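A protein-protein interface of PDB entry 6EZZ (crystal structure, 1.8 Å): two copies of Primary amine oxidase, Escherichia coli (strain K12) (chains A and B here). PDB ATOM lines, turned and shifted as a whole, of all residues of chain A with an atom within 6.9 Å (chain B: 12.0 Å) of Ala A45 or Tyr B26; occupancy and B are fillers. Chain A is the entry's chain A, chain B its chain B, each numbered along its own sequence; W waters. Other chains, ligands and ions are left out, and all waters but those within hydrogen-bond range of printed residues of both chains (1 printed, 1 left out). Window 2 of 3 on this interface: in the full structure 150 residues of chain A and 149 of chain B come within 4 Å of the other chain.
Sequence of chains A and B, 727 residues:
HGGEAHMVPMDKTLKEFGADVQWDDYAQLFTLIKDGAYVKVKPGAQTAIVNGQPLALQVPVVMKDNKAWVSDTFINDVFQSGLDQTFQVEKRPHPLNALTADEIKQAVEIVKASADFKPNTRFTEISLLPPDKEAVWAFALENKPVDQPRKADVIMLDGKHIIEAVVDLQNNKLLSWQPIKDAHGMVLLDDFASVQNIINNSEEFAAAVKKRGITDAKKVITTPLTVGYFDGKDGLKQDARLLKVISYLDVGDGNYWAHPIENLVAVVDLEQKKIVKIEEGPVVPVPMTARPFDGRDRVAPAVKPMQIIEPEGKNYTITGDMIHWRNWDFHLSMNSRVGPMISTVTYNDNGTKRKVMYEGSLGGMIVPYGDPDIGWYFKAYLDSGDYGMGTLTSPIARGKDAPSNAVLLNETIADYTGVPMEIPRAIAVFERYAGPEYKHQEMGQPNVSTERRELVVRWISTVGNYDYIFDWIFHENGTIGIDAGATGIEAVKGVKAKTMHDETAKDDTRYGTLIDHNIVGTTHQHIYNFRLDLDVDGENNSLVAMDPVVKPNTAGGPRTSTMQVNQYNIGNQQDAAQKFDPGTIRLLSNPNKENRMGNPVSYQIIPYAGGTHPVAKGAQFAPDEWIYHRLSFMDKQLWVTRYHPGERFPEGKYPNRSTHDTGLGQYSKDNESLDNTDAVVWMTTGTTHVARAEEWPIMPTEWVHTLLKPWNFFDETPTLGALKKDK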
ATOM      1  N   LEU A  29      -9.373  21.248 -26.534  1.00  0.00           N
ATOM      2  CA  LEU A  29      -8.411  20.751 -27.525  1.00  0.00           C
ATOM      3  C   LEU A  29      -7.712  21.912 -28.177  1.00  0.00           C
ATOM      4  O   LEU A  29      -8.380  22.862 -28.680  1.00  0.00           O
ATOM      5  CB  LEU A  29      -9.133  19.944 -28.588  1.00  0.00           C
ATOM      6  CG  LEU A  29      -8.220  19.311 -29.667  1.00  0.00           C
ATOM      7  CD1 LEU A  29      -7.461  18.141 -29.069  1.00  0.00           C
ATOM      8  CD2 LEU A  29      -9.074  18.846 -30.842  1.00  0.00           C
ATOM      9  N   PHE A  30      -6.383  21.850 -28.174  1.00  0.00           N
ATOM     10  CA  PHE A  30      -5.550  22.729 -28.986  1.00  0.00           C
ATOM     11  C   PHE A  30      -5.291  22.035 -30.340  1.00  0.00           C
ATOM     12  O   PHE A  30      -4.971  20.818 -30.365  1.00  0.00           O
ATOM     13  CB  PHE A  30      -4.195  23.009 -28.368  1.00  0.00           C
ATOM     14  CG  PHE A  30      -4.222  23.990 -27.249  1.00  0.00           C
ATOM     15  CD1 PHE A  30      -4.359  25.334 -27.517  1.00  0.00           C
ATOM     16  CD2 PHE A  30      -4.100  23.563 -25.946  1.00  0.00           C
ATOM     17  CE1 PHE A  30      -4.370  26.261 -26.506  1.00  0.00           C
ATOM     18  CE2 PHE A  30      -4.150  24.488 -24.910  1.00  0.00           C
ATOM     19  CZ  PHE A  30      -4.261  25.844 -25.204  1.00  0.00           C
ATOM     20  N   LYS A  40      -2.762  17.826 -32.684  1.00  0.00           N
ATOM     21  CA  LYS A  40      -3.861  17.947 -31.698  1.00  0.00           C
ATOM     22  C   LYS A  40      -3.343  17.556 -30.317  1.00  0.00           C
ATOM     23  O   LYS A  40      -2.658  16.545 -30.158  1.00  0.00           O
ATOM     24  CB  LYS A  40      -5.040  17.099 -32.086  1.00  0.00           C
ATOM     25  CG  LYS A  40      -5.645  17.570 -33.396  1.00  0.00           C
ATOM     26  CD  LYS A  40      -6.871  16.805 -33.843  1.00  0.00           C
ATOM     27  CE  LYS A  40      -6.552  15.421 -34.313  1.00  0.00           C
ATOM     28  NZ  LYS A  40      -7.670  14.948 -35.187  1.00  0.00           N
ATOM     29  N   VAL A  41      -3.657  18.369 -29.317  1.00  0.00           N
ATOM     30  CA  VAL A  41      -3.190  18.106 -27.956  1.00  0.00           C
ATOM     31  C   VAL A  41      -4.194  18.653 -26.919  1.00  0.00           C
ATOM     32  O   VAL A  41      -4.630  19.799 -27.026  1.00  0.00           O
ATOM     33  CB  VAL A  41      -1.748  18.624 -27.704  1.00  0.00           C
ATOM     34  CG1 VAL A  41      -1.601  20.145 -27.851  1.00  0.00           C
ATOM     35  CG2 VAL A  41      -1.236  18.132 -26.330  1.00  0.00           C
ATOM     36  N   LYS A  42      -4.596  17.797 -25.991  1.00  0.00           N
ATOM     37  CA  LYS A  42      -5.450  18.194 -24.867  1.00  0.00           C
ATOM     38  C   LYS A  42      -4.589  18.496 -23.626  1.00  0.00           C
ATOM     39  O   LYS A  42      -3.642  17.768 -23.325  1.00  0.00           O
ATOM     40  CB  LYS A  42      -6.433  17.100 -24.539  1.00  0.00           C
ATOM     41  CG  LYS A  42      -7.403  16.731 -25.642  1.00  0.00           C
ATOM     42  CD  LYS A  42      -7.878  15.303 -25.476  1.00  0.00           C
ATOM     43  CE  LYS A  42      -8.580  15.053 -24.132  1.00  0.00           C
ATOM     44  NZ  LYS A  42      -9.732  15.974 -23.932  1.00  0.00           N
ATOM     45  N   PRO A  43      -4.924  19.557 -22.879  1.00  0.00           N
ATOM     46  CA  PRO A  43      -4.267  19.824 -21.585  1.00  0.00           C
ATOM     47  C   PRO A  43      -4.365  18.621 -20.654  1.00  0.00           C
ATOM     48  O   PRO A  43      -5.394  17.931 -20.610  1.00  0.00           O
ATOM     49  CB  PRO A  43      -5.073  20.993 -21.009  1.00  0.00           C
ATOM     50  CG  PRO A  43      -5.706  21.639 -22.210  1.00  0.00           C
ATOM     51  CD  PRO A  43      -6.021  20.507 -23.135  1.00  0.00           C
ATOM     52  N   GLY A  44      -3.262  18.325 -19.997  1.00  0.00           N
ATOM     53  CA  GLY A  44      -3.183  17.203 -19.086  1.00  0.00           C
ATOM     54  C   GLY A  44      -2.996  15.858 -19.754  1.00  0.00           C
ATOM     55  O   GLY A  44      -2.768  14.872 -19.062  1.00  0.00           O
ATOM     56  N   ALA A  45      -3.095  15.764 -21.081  1.00  0.00           N
ATOM     57  CA  ALA A  45      -3.050  14.420 -21.715  1.00  0.00           C
ATOM     58  C   ALA A  45      -1.601  13.934 -21.801  1.00  0.00           C
ATOM     59  O   ALA A  45      -0.694  14.726 -21.958  1.00  0.00           O
ATOM     60  CB  ALA A  45      -3.692  14.404 -23.094  1.00  0.00           C
ATOM     61  N   GLN A  46      -1.408  12.622 -21.661  1.00  0.00           N
ATOM     62  CA  GLN A  46      -0.061  12.040 -21.716  1.00  0.00           C
ATOM     63  C   GLN A  46       0.410  11.810 -23.156  1.00  0.00           C
ATOM     64  O   GLN A  46       1.601  11.543 -23.389  1.00  0.00           O
ATOM     65  CB  GLN A  46      -0.042  10.718 -20.940  1.00  0.00           C
ATOM     66  CG  GLN A  46      -0.161  10.851 -19.420  1.00  0.00           C
ATOM     67  CD  GLN A  46      -0.295   9.487 -18.719  1.00  0.00           C
ATOM     68  OE1 GLN A  46       0.116   8.435 -19.235  1.00  0.00           O
ATOM     69  NE2 GLN A  46      -0.888   9.502 -17.542  1.00  0.00           N
ATOM     70  N   THR A  47      -0.507  11.926 -24.110  1.00  0.00           N
ATOM     71  CA  THR A  47      -0.208  11.802 -25.539  1.00  0.00           C
ATOM     72  C   THR A  47      -0.805  12.957 -26.363  1.00  0.00           C
ATOM     73  O   THR A  47      -1.710  13.643 -25.916  1.00  0.00           O
ATOM     74  CB  THR A  47      -0.726  10.489 -26.138  1.00  0.00           C
ATOM     75  OG1 THR A  47      -2.149  10.514 -26.238  1.00  0.00           O
ATOM     76  CG2 THR A  47      -0.305   9.295 -25.328  1.00  0.00           C
ATOM     77  N   ALA A  48      -0.250  13.138 -27.554  1.00  0.00           N
ATOM     78  CA  ALA A  48      -0.744  14.071 -28.571  1.00  0.00           C
ATOM     79  C   ALA A  48      -0.945  13.332 -29.894  1.00  0.00           C
ATOM     80  O   ALA A  48      -0.660  12.118 -29.994  1.00  0.00           O
ATOM     81  CB  ALA A  48       0.242  15.204 -28.699  1.00  0.00           C
ATOM     82  N   ILE A  49      -1.529  14.001 -30.886  1.00  0.00           N
ATOM     83  CA  ILE A  49      -1.638  13.449 -32.248  1.00  0.00           C
ATOM     84  C   ILE A  49      -0.852  14.340 -33.197  1.00  0.00           C
ATOM     85  O   ILE A  49      -1.053  15.570 -33.192  1.00  0.00           O
ATOM     86  CB  ILE A  49      -3.108  13.383 -32.701  1.00  0.00           C
ATOM     87  CG1 ILE A  49      -3.920  12.506 -31.759  1.00  0.00           C
ATOM     88  CG2 ILE A  49      -3.234  12.907 -34.164  1.00  0.00           C
ATOM     89  CD1 ILE A  49      -3.581  11.025 -31.827  1.00  0.00           C
ATOM     90  N   LEU A  55       1.610  10.262 -30.271  1.00  0.00           N
ATOM     91  CA  LEU A  55       2.918  10.657 -29.769  1.00  0.00           C
ATOM     92  C   LEU A  55       2.877  10.689 -28.246  1.00  0.00           C
ATOM     93  O   LEU A  55       2.045  11.405 -27.672  1.00  0.00           O
ATOM     94  CB  LEU A  55       3.274  12.073 -30.233  1.00  0.00           C
ATOM     95  CG  LEU A  55       4.644  12.606 -29.791  1.00  0.00           C
ATOM     96  CD1 LEU A  55       5.767  11.800 -30.460  1.00  0.00           C
ATOM     97  CD2 LEU A  55       4.782  14.098 -30.061  1.00  0.00           C
ATOM     98  N   LEU A  57       4.058  12.073 -24.754  1.00  0.00           N
ATOM     99  CA  LEU A  57       4.669  13.305 -24.316  1.00  0.00           C
ATOM    100  C   LEU A  57       5.469  13.035 -23.022  1.00  0.00           C
ATOM    101  O   LEU A  57       4.988  12.366 -22.159  1.00  0.00           O
ATOM    102  CB  LEU A  57       3.594  14.358 -24.045  1.00  0.00           C
ATOM    103  CG  LEU A  57       2.726  14.748 -25.231  1.00  0.00           C
ATOM    104  CD1 LEU A  57       1.585  15.627 -24.744  1.00  0.00           C
ATOM    105  CD2 LEU A  57       3.575  15.451 -26.275  1.00  0.00           C
ATOM    106  N   VAL A  59       6.151  15.563 -20.954  1.00  0.00           N
ATOM    107  CA  VAL A  59       5.526  16.532 -20.053  1.00  0.00           C
ATOM    108  C   VAL A  59       4.175  16.980 -20.670  1.00  0.00           C
ATOM    109  O   VAL A  59       4.185  17.592 -21.725  1.00  0.00           O
ATOM    110  CB  VAL A  59       6.443  17.758 -19.849  1.00  0.00           C
ATOM    111  CG1 VAL A  59       5.758  18.793 -18.959  1.00  0.00           C
ATOM    112  CG2 VAL A  59       7.787  17.355 -19.248  1.00  0.00           C
ATOM    113  N   PRO A  60       3.031  16.641 -20.040  1.00  0.00           N
ATOM    114  CA  PRO A  60       1.750  17.129 -20.542  1.00  0.00           C
ATOM    115  C   PRO A  60       1.683  18.661 -20.671  1.00  0.00           C
ATOM    116  O   PRO A  60       2.459  19.383 -20.013  1.00  0.00           O
ATOM    117  CB  PRO A  60       0.761  16.614 -19.509  1.00  0.00           C
ATOM    118  CG  PRO A  60       1.371  15.310 -19.071  1.00  0.00           C
ATOM    119  CD  PRO A  60       2.835  15.630 -18.983  1.00  0.00           C
ATOM    120  N   VAL A  61       0.803  19.139 -21.558  1.00  0.00           N
ATOM    121  CA  VAL A  61       0.487  20.563 -21.617  1.00  0.00           C
ATOM    122  C   VAL A  61      -0.189  20.895 -20.276  1.00  0.00           C
ATOM    123  O   VAL A  61      -1.082  20.180 -19.874  1.00  0.00           O
ATOM    124  CB  VAL A  61      -0.485  20.875 -22.759  1.00  0.00           C
ATOM    125  CG1 VAL A  61      -1.003  22.329 -22.668  1.00  0.00           C
ATOM    126  CG2 VAL A  61       0.166  20.597 -24.102  1.00  0.00           C
ATOM    127  N   GLN B  22     -17.363  12.738 -39.164  1.00  0.00           N
ATOM    128  CA  GLN B  22     -15.982  12.428 -38.776  1.00  0.00           C
ATOM    129  C   GLN B  22     -15.924  12.158 -37.288  1.00  0.00           C
ATOM    130  O   GLN B  22     -16.491  12.914 -36.488  1.00  0.00           O
ATOM    131  CB  GLN B  22     -15.007  13.575 -39.079  1.00  0.00           C
ATOM    132  CG  GLN B  22     -15.002  14.082 -40.520  1.00  0.00           C
ATOM    133  CD  GLN B  22     -14.102  13.297 -41.477  1.00  0.00           C
ATOM    134  OE1 GLN B  22     -12.936  13.032 -41.181  1.00  0.00           O
ATOM    135  NE2 GLN B  22     -14.646  12.942 -42.652  1.00  0.00           N
ATOM    136  N   TRP B  23     -15.238  11.078 -36.921  1.00  0.00           N
ATOM    137  CA  TRP B  23     -15.047  10.690 -35.536  1.00  0.00           C
ATOM    138  C   TRP B  23     -13.593  10.862 -35.200  1.00  0.00           C
ATOM    139  O   TRP B  23     -12.747  10.322 -35.893  1.00  0.00           O
ATOM    140  CB  TRP B  23     -15.442   9.212 -35.341  1.00  0.00           C
ATOM    141  CG  TRP B  23     -15.029   8.654 -34.008  1.00  0.00           C
ATOM    142  CD1 TRP B  23     -14.149   7.636 -33.800  1.00  0.00           C
ATOM    143  CD2 TRP B  23     -15.442   9.099 -32.703  1.00  0.00           C
ATOM    144  NE1 TRP B  23     -14.019   7.390 -32.455  1.00  0.00           N
ATOM    145  CE2 TRP B  23     -14.777   8.288 -31.757  1.00  0.00           C
ATOM    146  CE3 TRP B  23     -16.312  10.096 -32.241  1.00  0.00           C
ATOM    147  CZ2 TRP B  23     -14.958   8.429 -30.385  1.00  0.00           C
ATOM    148  CZ3 TRP B  23     -16.493  10.240 -30.881  1.00  0.00           C
ATOM    149  CH2 TRP B  23     -15.815   9.412 -29.961  1.00  0.00           C
ATOM    150  N   ASP B  24     -13.305  11.606 -34.138  1.00  0.00           N
ATOM    151  CA  ASP B  24     -11.944  11.790 -33.638  1.00  0.00           C
ATOM    152  C   ASP B  24     -11.843  11.070 -32.288  1.00  0.00           C
ATOM    153  O   ASP B  24     -12.344  11.534 -31.248  1.00  0.00           O
ATOM    154  CB  ASP B  24     -11.639  13.282 -33.495  1.00  0.00           C
ATOM    155  CG  ASP B  24     -10.202  13.562 -33.088  1.00  0.00           C
ATOM    156  OD1 ASP B  24      -9.503  12.685 -32.507  1.00  0.00           O
ATOM    157  OD2 ASP B  24      -9.752  14.703 -33.325  1.00  0.00           O
ATOM    158  N   ASP B  25     -11.121   9.962 -32.307  1.00  0.00           N
ATOM    159  CA  ASP B  25     -10.961   9.097 -31.143  1.00  0.00           C
ATOM    160  C   ASP B  25     -10.107   9.711 -30.022  1.00  0.00           C
ATOM    161  O   ASP B  25     -10.350   9.466 -28.835  1.00  0.00           O
ATOM    162  CB  ASP B  25     -10.380   7.734 -31.593  1.00  0.00           C
ATOM    163  CG  ASP B  25     -10.586   6.658 -30.557  1.00  0.00           C
ATOM    164  OD1 ASP B  25     -11.749   6.219 -30.376  1.00  0.00           O
ATOM    165  OD2 ASP B  25      -9.589   6.278 -29.914  1.00  0.00           O
ATOM    166  N   TYR B  26      -9.150  10.545 -30.386  1.00  0.00           N
ATOM    167  CA  TYR B  26      -8.314  11.214 -29.397  1.00  0.00           C
ATOM    168  C   TYR B  26      -9.132  12.288 -28.650  1.00  0.00           C
ATOM    169  O   TYR B  26      -9.059  12.391 -27.423  1.00  0.00           O
ATOM    170  CB  TYR B  26      -7.110  11.876 -30.045  1.00  0.00           C
ATOM    171  CG  TYR B  26      -6.249  12.714 -29.129  1.00  0.00           C
ATOM    172  CD1 TYR B  26      -5.400  12.117 -28.198  1.00  0.00           C
ATOM    173  CD2 TYR B  26      -6.263  14.093 -29.196  1.00  0.00           C
ATOM    174  CE1 TYR B  26      -4.587  12.867 -27.398  1.00  0.00           C
ATOM    175  CE2 TYR B  26      -5.432  14.862 -28.412  1.00  0.00           C
ATOM    176  CZ  TYR B  26      -4.599  14.252 -27.485  1.00  0.00           C
ATOM    177  OH  TYR B  26      -3.778  15.022 -26.695  1.00  0.00           O
ATOM    178  N   ALA B  27      -9.891  13.080 -29.398  1.00  0.00           N
ATOM    179  CA  ALA B  27     -10.683  14.202 -28.807  1.00  0.00           C
ATOM    180  C   ALA B  27     -12.035  13.725 -28.285  1.00  0.00           C
ATOM    181  O   ALA B  27     -12.714  14.480 -27.613  1.00  0.00           O
ATOM    182  CB  ALA B  27     -10.895  15.285 -29.873  1.00  0.00           C
ATOM    183  N   GLN B  28     -12.433  12.486 -28.626  1.00  0.00           N
ATOM    184  CA  GLN B  28     -13.758  11.934 -28.354  1.00  0.00           C
ATOM    185  C   GLN B  28     -14.842  12.853 -28.909  1.00  0.00           C
ATOM    186  O   GLN B  28     -15.802  13.212 -28.214  1.00  0.00           O
ATOM    187  CB  GLN B  28     -13.956  11.609 -26.862  1.00  0.00           C
ATOM    188  CG  GLN B  28     -13.033  10.494 -26.369  1.00  0.00           C
ATOM    189  CD  GLN B  28     -13.478   9.132 -26.812  1.00  0.00           C
ATOM    190  OE1 GLN B  28     -14.595   8.741 -26.525  1.00  0.00           O
ATOM    191  NE2 GLN B  28     -12.601   8.391 -27.539  1.00  0.00           N
ATOM    192  N   LEU B  29     -14.660  13.219 -30.185  1.00  0.00           N
ATOM    193  CA  LEU B  29     -15.429  14.295 -30.812  1.00  0.00           C
ATOM    194  C   LEU B  29     -15.923  13.871 -32.182  1.00  0.00           C
ATOM    195  O   LEU B  29     -15.112  13.454 -33.021  1.00  0.00           O
ATOM    196  CB  LEU B  29     -14.544  15.547 -30.952  1.00  0.00           C
ATOM    197  CG  LEU B  29     -15.199  16.810 -31.551  1.00  0.00           C
ATOM    198  CD1 LEU B  29     -16.233  17.367 -30.600  1.00  0.00           C
ATOM    199  CD2 LEU B  29     -14.140  17.878 -31.839  1.00  0.00           C
ATOM    200  N   PHE B  30     -17.230  13.993 -32.406  1.00  0.00           N
ATOM    201  CA  PHE B  30     -17.811  13.974 -33.760  1.00  0.00           C
ATOM    202  C   PHE B  30     -17.832  15.368 -34.396  1.00  0.00           C
ATOM    203  O   PHE B  30     -18.244  16.340 -33.760  1.00  0.00           O
ATOM    204  CB  PHE B  30     -19.246  13.469 -33.735  1.00  0.00           C
ATOM    205  CG  PHE B  30     -19.368  11.986 -33.543  1.00  0.00           C
ATOM    206  CD1 PHE B  30     -19.107  11.120 -34.596  1.00  0.00           C
ATOM    207  CD2 PHE B  30     -19.760  11.473 -32.349  1.00  0.00           C
ATOM    208  CE1 PHE B  30     -19.227   9.746 -34.445  1.00  0.00           C
ATOM    209  CE2 PHE B  30     -19.869  10.089 -32.169  1.00  0.00           C
ATOM    210  CZ  PHE B  30     -19.596   9.224 -33.222  1.00  0.00           C
ATOM    211  N   THR B  31     -17.421  15.453 -35.652  1.00  0.00           N
ATOM    212  CA  THR B  31     -17.637  16.643 -36.455  1.00  0.00           C
ATOM    213  C   THR B  31     -18.583  16.265 -37.592  1.00  0.00           C
ATOM    214  O   THR B  31     -18.336  15.307 -38.349  1.00  0.00           O
ATOM    215  CB  THR B  31     -16.310  17.221 -36.966  1.00  0.00           C
ATOM    216  OG1 THR B  31     -15.465  17.528 -35.848  1.00  0.00           O
ATOM    217  CG2 THR B  31     -16.541  18.495 -37.786  1.00  0.00           C
ATOM    218  N   VAL B  41     -20.021  17.583 -31.662  1.00  0.00           N
ATOM    219  CA  VAL B  41     -20.734  16.921 -30.569  1.00  0.00           C
ATOM    220  C   VAL B  41     -19.906  15.781 -29.964  1.00  0.00           C
ATOM    221  O   VAL B  41     -19.306  14.992 -30.694  1.00  0.00           O
ATOM    222  CB  VAL B  41     -22.145  16.459 -30.988  1.00  0.00           C
ATOM    223  CG1 VAL B  41     -22.096  15.421 -32.095  1.00  0.00           C
ATOM    224  CG2 VAL B  41     -22.931  15.926 -29.801  1.00  0.00           C
ATOM    225  N   LYS B  42     -19.844  15.751 -28.627  1.00  0.00           N
ATOM    226  CA  LYS B  42     -19.146  14.700 -27.869  1.00  0.00           C
ATOM    227  C   LYS B  42     -20.174  13.709 -27.339  1.00  0.00           C
ATOM    228  O   LYS B  42     -21.237  14.128 -26.850  1.00  0.00           O
ATOM    229  CB  LYS B  42     -18.354  15.292 -26.683  1.00  0.00           C
ATOM    230  CG  LYS B  42     -17.204  16.193 -27.092  1.00  0.00           C
ATOM    231  CD  LYS B  42     -16.493  16.887 -25.938  1.00  0.00           C
ATOM    232  CE  LYS B  42     -15.878  15.947 -24.923  1.00  0.00           C
ATOM    233  NZ  LYS B  42     -14.957  14.980 -25.547  1.00  0.00           N
ATOM    234  N   PRO B  43     -19.878  12.392 -27.411  1.00  0.00           N
ATOM    235  CA  PRO B  43     -20.760  11.400 -26.752  1.00  0.00           C
ATOM    236  C   PRO B  43     -21.026  11.777 -25.314  1.00  0.00           C
ATOM    237  O   PRO B  43     -20.124  12.255 -24.625  1.00  0.00           O
ATOM    238  CB  PRO B  43     -19.946  10.106 -26.781  1.00  0.00           C
ATOM    239  CG  PRO B  43     -18.928  10.300 -27.853  1.00  0.00           C
ATOM    240  CD  PRO B  43     -18.696  11.766 -28.029  1.00  0.00           C
ATOM    241  N   MET B  63     -22.650   6.428 -26.991  1.00  0.00           N
ATOM    242  CA  MET B  63     -21.651   5.499 -27.505  1.00  0.00           C
ATOM    243  C   MET B  63     -21.826   4.194 -26.734  1.00  0.00           C
ATOM    244  O   MET B  63     -22.136   4.201 -25.542  1.00  0.00           O
ATOM    245  CB  MET B  63     -20.249   6.082 -27.340  1.00  0.00           C
ATOM    246  CG  MET B  63     -19.192   5.392 -28.182  1.00  0.00           C
ATOM    247  SD  MET B  63     -19.437   5.588 -29.958  1.00  0.00           S
ATOM    248  CE  MET B  63     -18.202   6.816 -30.367  1.00  0.00           C
ATOM    249  N   ASN B  66     -18.410   0.711 -29.198  1.00  0.00           N
ATOM    250  CA  ASN B  66     -17.871   1.477 -30.331  1.00  0.00           C
ATOM    251  C   ASN B  66     -18.911   1.859 -31.395  1.00  0.00           C
ATOM    252  O   ASN B  66     -18.573   2.023 -32.557  1.00  0.00           O
ATOM    253  CB  ASN B  66     -16.698   0.729 -30.978  1.00  0.00           C
ATOM    254  CG  ASN B  66     -15.509   0.603 -30.054  1.00  0.00           C
ATOM    255  OD1 ASN B  66     -15.033   1.595 -29.503  1.00  0.00           O
ATOM    256  ND2 ASN B  66     -15.004  -0.616 -29.898  1.00  0.00           N
HETATM  257  O   HOH W   1     -11.372  16.274 -26.136  1.00  0.00           O
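The backbone carbonyl oxygen (O) of Thr A47 is in hydrogen-bond range of the side-chain hydroxyl (OH) of Tyr B26.
NZ of Lys A40 lies within salt-bridge range of OD2 of Asp B24 (2.8 Å).
The side-chain hydroxyl (OH) of Tyr B26 sits at hydrogen-bond distance from the backbone NH (N) of Lys A42 (3.0 Å).
The backbone NH (N) of Asp B24 lies within hydrogen-bond range of the backbone carbonyl oxygen (O) of Leu B29.
The backbone NH of Lys A40 is in hydrogen-bond range of the backbone carbonyl oxygen of Ile A49 (2.9 Å).
N of Ala A48 lies within hydrogen-bond range of O of Leu A55, 2.9 Å away.
The backbone NH (N) of Phe A30 lies within hydrogen-bond range of the backbone carbonyl oxygen (O) of Val A41 (2.9 Å).
The side-chain carboxylate (OD1) of Asp B24 lies within hydrogen-bond range of the backbone NH (N) of Tyr B26 (3.0 Å).
OD1 of Asp B24 is in hydrogen-bond range of N of Ala B27, 3.2 Å away.
Leu A29 touches Tyr B26 (CD1 to CE2, 3.9 Å).
Lys A40 touches Tyr B26 (O to CE2, 3.7 Å).
CA of Val A41 touches OH of Tyr B26, at 3.4 Å.
Tyr B26 touches Ala A45 (OH to CB, 3.7 Å).
Tyr B26 touches Ala A48 (OH to CA, 3.7 Å).
Ile A49 touches Tyr B26.
Ala A45 touches just one residue of chain B: Tyr B26 (3.7 Å).
Tyr B26 touches eight residues of chain A.
Of the printed residues of chain B, Lys A40 touches Asp B24 (2.8 Å) and Tyr B26 (3.7 Å).
Of the printed residues of chain B, Val A41 touches Tyr B26 (3.4 Å).
Lys A42 touches one residue of chain B.
No residue of chain B comes within 4 Å of Pro A43.
No residue of chain B comes within 4 Å of Gly A44.
No residue of chain B comes within 4 Å of Gln A46.
Thr A47 touches just one residue of chain B: Tyr B26 (2.6 Å).
Ala A48 touches just one residue of chain B: Tyr B26 (3.7 Å).
Ile A49 touches just one residue of chain B: Tyr B26 (3.5 Å).
No residue of chain B comes within 4 Å of Leu A57.
No residue of chain B comes within 4 Å of Val A61.
Printed residues of chain B within 4 Å of Leu A29: Tyr B26.
Of the printed residues of chain A, Asp B24 touches Lys A40 (2.8 Å).
The nearest residue of chain B that does not touch Ala A45 is Ala B27 (8.9 Å).
The nearest residue of chain A that does not touch Tyr B26 is Leu A57 (5.7 Å).
The nearest printed residue of chain B that does not touch Leu A29 is Ala B27 (4.1 Å).
Printed residues of chain B that touch a printed residue of chain A: Asp B24 and Tyr B26.
Hydrophobic or aromatic side chains of chain B that line the printed part of chain A: Tyr B26.
5 positions are printed for both chains.
Of the 9 pairs that touch across the chains among the printed residues, none has its exchanged pair printed and touching as well.
Water W1 bridges the backbone carbonyl oxygen of Ala B27 (2.7 Å) and the side-chain amino group of Lys A42 (2.8 Å).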
